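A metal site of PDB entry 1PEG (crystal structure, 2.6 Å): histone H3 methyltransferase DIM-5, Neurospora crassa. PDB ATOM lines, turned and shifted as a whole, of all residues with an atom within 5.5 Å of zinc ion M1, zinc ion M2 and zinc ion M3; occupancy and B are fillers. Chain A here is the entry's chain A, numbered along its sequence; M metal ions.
The side-chain sulfur (SG) of Cys 63 lies close to the backbone NH (N) of Cys 65, 3.7 Å away. SG of Cys 122 sits close to N of Asn 124 (3.4 Å). The backbone carbonyl oxygen (O) of Asn 124 sits at hydrogen-bond distance from the backbone NH (N) of Cys 112, 2.8 Å away. SG of Cys 116 lies close to N of His 113.
Four residues have an atom within 4 Å of zinc ion M2: Cys 50, Cys 65, Cys 112 and Cys 116. The nearest printed residue that does not touch zinc ion M2 is Cys 63 (4.1 Å).
Of the 15 residues printed, 5 come within 4 Å of zinc ion M3. The nearest printed residue that does not touch zinc ion M3 is Cys 116 (4.6 Å).
Zinc ion M1 is bound by the side-chain sulfur of Cys 50 (2.3 Å), the side-chain sulfur of Cys 58 (2.3 Å), the side-chain sulfur of Cys 63 (2.3 Å) and the side-chain sulfur of Cys 52 (2.3 Å). Zinc ion M1 has four donor atoms within binding distance.
Zinc ion M2 is bound by SG of Cys 65, SG of Cys 50, SG of Cys 116 and SG of Cys 112.
The side-chain sulfur (SG) of Cys 58 binds zinc ion M3 (2.2 Å). SG of Cys 118 is bound to zinc ion M3 (2.3 Å). SG of Cys 122 is bound to zinc ion M3 (2.3 Å). SG of Cys 112 is bound to zinc ion M3 (2.3 Å). Zinc ion M3 has four donor atoms within binding distance.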
ATOM      1  N   GLY A  49      10.322  -2.479   1.833  1.00  0.00           N
ATOM      2  CA  GLY A  49       9.095  -3.112   1.434  1.00  0.00           C
ATOM      3  C   GLY A  49       8.178  -2.897   2.600  1.00  0.00           C
ATOM      4  O   GLY A  49       8.433  -2.048   3.443  1.00  0.00           O
ATOM      5  N   CYS A  50       7.098  -3.669   2.671  1.00  0.00           N
ATOM      6  CA  CYS A  50       6.164  -3.566   3.787  1.00  0.00           C
ATOM      7  C   CYS A  50       6.173  -4.804   4.705  1.00  0.00           C
ATOM      8  O   CYS A  50       6.191  -5.945   4.253  1.00  0.00           O
ATOM      9  CB  CYS A  50       4.740  -3.239   3.282  1.00  0.00           C
ATOM     10  SG  CYS A  50       3.916  -4.488   2.248  1.00  0.00           S
ATOM     11  N   CYS A  52       3.872  -5.650   6.620  1.00  0.00           N
ATOM     12  CA  CYS A  52       2.529  -6.169   6.706  1.00  0.00           C
ATOM     13  C   CYS A  52       2.618  -7.654   7.022  1.00  0.00           C
ATOM     14  O   CYS A  52       3.537  -8.353   6.590  1.00  0.00           O
ATOM     15  CB  CYS A  52       1.794  -6.001   5.363  1.00  0.00           C
ATOM     16  SG  CYS A  52       1.162  -4.333   5.010  1.00  0.00           S
ATOM     17  N   GLU A  57      -2.551  -7.499   3.806  1.00  0.00           N
ATOM     18  CA  GLU A  57      -3.566  -6.509   4.066  1.00  0.00           C
ATOM     19  C   GLU A  57      -2.928  -5.254   3.626  1.00  0.00           C
ATOM     20  O   GLU A  57      -2.785  -4.270   4.341  1.00  0.00           O
ATOM     21  CB  GLU A  57      -3.974  -6.451   5.537  1.00  0.00           C
ATOM     22  N   CYS A  58      -2.551  -5.326   2.337  1.00  0.00           N
ATOM     23  CA  CYS A  58      -1.836  -4.257   1.685  1.00  0.00           C
ATOM     24  C   CYS A  58      -2.809  -3.451   0.845  1.00  0.00           C
ATOM     25  O   CYS A  58      -2.427  -2.891  -0.183  1.00  0.00           O
ATOM     26  CB  CYS A  58      -0.713  -4.816   0.780  1.00  0.00           C
ATOM     27  SG  CYS A  58       0.618  -5.779   1.586  1.00  0.00           S
ATOM     28  N   CYS A  63      -0.169   0.246   5.237  1.00  0.00           N
ATOM     29  CA  CYS A  63       0.998  -0.251   4.461  1.00  0.00           C
ATOM     30  C   CYS A  63       1.832   0.931   3.944  1.00  0.00           C
ATOM     31  O   CYS A  63       1.300   1.858   3.326  1.00  0.00           O
ATOM     32  CB  CYS A  63       0.473  -1.127   3.303  1.00  0.00           C
ATOM     33  SG  CYS A  63       1.683  -1.902   2.169  1.00  0.00           S
ATOM     34  N   GLN A  64       3.140   0.893   4.203  1.00  0.00           N
ATOM     35  CA  GLN A  64       4.058   1.963   3.792  1.00  0.00           C
ATOM     36  C   GLN A  64       4.289   2.059   2.288  1.00  0.00           C
ATOM     37  O   GLN A  64       4.952   2.983   1.822  1.00  0.00           O
ATOM     38  CB  GLN A  64       5.411   1.796   4.501  1.00  0.00           C
ATOM     39  N   CYS A  65       3.736   1.110   1.538  1.00  0.00           N
ATOM     40  CA  CYS A  65       3.880   1.081   0.079  1.00  0.00           C
ATOM     41  C   CYS A  65       3.026   2.163  -0.584  1.00  0.00           C
ATOM     42  O   CYS A  65       3.330   2.631  -1.682  1.00  0.00           O
ATOM     43  CB  CYS A  65       3.507  -0.323  -0.429  1.00  0.00           C
ATOM     44  SG  CYS A  65       4.765  -1.580  -0.007  1.00  0.00           S
ATOM     45  N   GLU A 111       2.708  -0.409  -6.158  1.00  0.00           N
ATOM     46  CA  GLU A 111       2.547  -1.844  -5.952  1.00  0.00           C
ATOM     47  C   GLU A 111       3.597  -2.386  -5.004  1.00  0.00           C
ATOM     48  O   GLU A 111       4.609  -1.737  -4.742  1.00  0.00           O
ATOM     49  CB  GLU A 111       2.661  -2.556  -7.285  1.00  0.00           C
ATOM     50  CG  GLU A 111       1.449  -3.337  -7.716  1.00  0.00           C
ATOM     51  CD  GLU A 111       1.717  -4.098  -9.002  1.00  0.00           C
ATOM     52  OE1 GLU A 111       1.382  -5.296  -9.100  1.00  0.00           O
ATOM     53  OE2 GLU A 111       2.286  -3.486  -9.910  1.00  0.00           O
ATOM     54  N   CYS A 112       3.340  -3.589  -4.485  1.00  0.00           N
ATOM     55  CA  CYS A 112       4.266  -4.245  -3.581  1.00  0.00           C
ATOM     56  C   CYS A 112       5.368  -4.927  -4.415  1.00  0.00           C
ATOM     57  O   CYS A 112       5.345  -4.832  -5.644  1.00  0.00           O
ATOM     58  CB  CYS A 112       3.520  -5.271  -2.716  1.00  0.00           C
ATOM     59  SG  CYS A 112       2.788  -4.563  -1.201  1.00  0.00           S
ATOM     60  N   HIS A 113       6.317  -5.586  -3.756  1.00  0.00           N
ATOM     61  CA  HIS A 113       7.433  -6.243  -4.444  1.00  0.00           C
ATOM     62  C   HIS A 113       8.138  -7.303  -3.581  1.00  0.00           C
ATOM     63  O   HIS A 113       7.532  -7.876  -2.682  1.00  0.00           O
ATOM     64  CB  HIS A 113       8.456  -5.199  -4.871  1.00  0.00           C
ATOM     65  CG  HIS A 113       8.714  -4.177  -3.826  1.00  0.00           C
ATOM     66  ND1 HIS A 113       8.270  -2.876  -3.916  1.00  0.00           N
ATOM     67  CD2 HIS A 113       9.328  -4.272  -2.622  1.00  0.00           C
ATOM     68  CE1 HIS A 113       8.602  -2.218  -2.827  1.00  0.00           C
ATOM     69  NE2 HIS A 113       9.249  -3.043  -2.024  1.00  0.00           N
ATOM     70  N   CYS A 116       8.493  -6.867   0.650  1.00  0.00           N
ATOM     71  CA  CYS A 116       7.432  -6.824   1.627  1.00  0.00           C
ATOM     72  C   CYS A 116       7.088  -8.175   2.238  1.00  0.00           C
ATOM     73  O   CYS A 116       7.290  -9.223   1.616  1.00  0.00           O
ATOM     74  CB  CYS A 116       6.194  -6.226   0.978  1.00  0.00           C
ATOM     75  SG  CYS A 116       6.578  -4.970  -0.262  1.00  0.00           S
ATOM     76  N   CYS A 118       4.603  -9.842   2.402  1.00  0.00           N
ATOM     77  CA  CYS A 118       3.366 -10.290   1.787  1.00  0.00           C
ATOM     78  C   CYS A 118       3.755 -11.152   0.582  1.00  0.00           C
ATOM     79  O   CYS A 118       4.868 -11.023   0.059  1.00  0.00           O
ATOM     80  CB  CYS A 118       2.522  -9.084   1.363  1.00  0.00           C
ATOM     81  SG  CYS A 118       3.206  -8.128  -0.020  1.00  0.00           S
ATOM     82  N   CYS A 122      -0.661 -10.981  -2.920  1.00  0.00           N
ATOM     83  CA  CYS A 122      -0.864  -9.660  -2.353  1.00  0.00           C
ATOM     84  C   CYS A 122      -1.647  -8.833  -3.374  1.00  0.00           C
ATOM     85  O   CYS A 122      -1.161  -8.508  -4.463  1.00  0.00           O
ATOM     86  CB  CYS A 122       0.449  -8.942  -2.040  1.00  0.00           C
ATOM     87  SG  CYS A 122       0.193  -7.148  -1.757  1.00  0.00           S
ATOM     88  N   ASN A 124      -2.109  -6.024  -4.065  1.00  0.00           N
ATOM     89  CA  ASN A 124      -1.477  -4.846  -4.647  1.00  0.00           C
ATOM     90  C   ASN A 124      -0.198  -5.205  -5.349  1.00  0.00           C
ATOM     91  O   ASN A 124       0.773  -4.472  -5.281  1.00  0.00           O
ATOM     92  CB  ASN A 124      -1.178  -3.844  -3.553  1.00  0.00           C
ATOM     93  CG  ASN A 124      -0.861  -2.470  -4.090  1.00  0.00           C
ATOM     94  OD1 ASN A 124      -0.962  -2.240  -5.284  1.00  0.00           O
ATOM     95  ND2 ASN A 124      -0.482  -1.553  -3.207  1.00  0.00           N
HETATM   96 ZN    ZN M   1       1.714  -4.130   2.742  1.00  0.00          ZN
HETATM   97 ZN    ZN M   2       4.611  -3.855   0.154  1.00  0.00          ZN
HETATM   98 ZN    ZN M   3       1.747  -6.380  -0.254  1.00  0.00          ZN
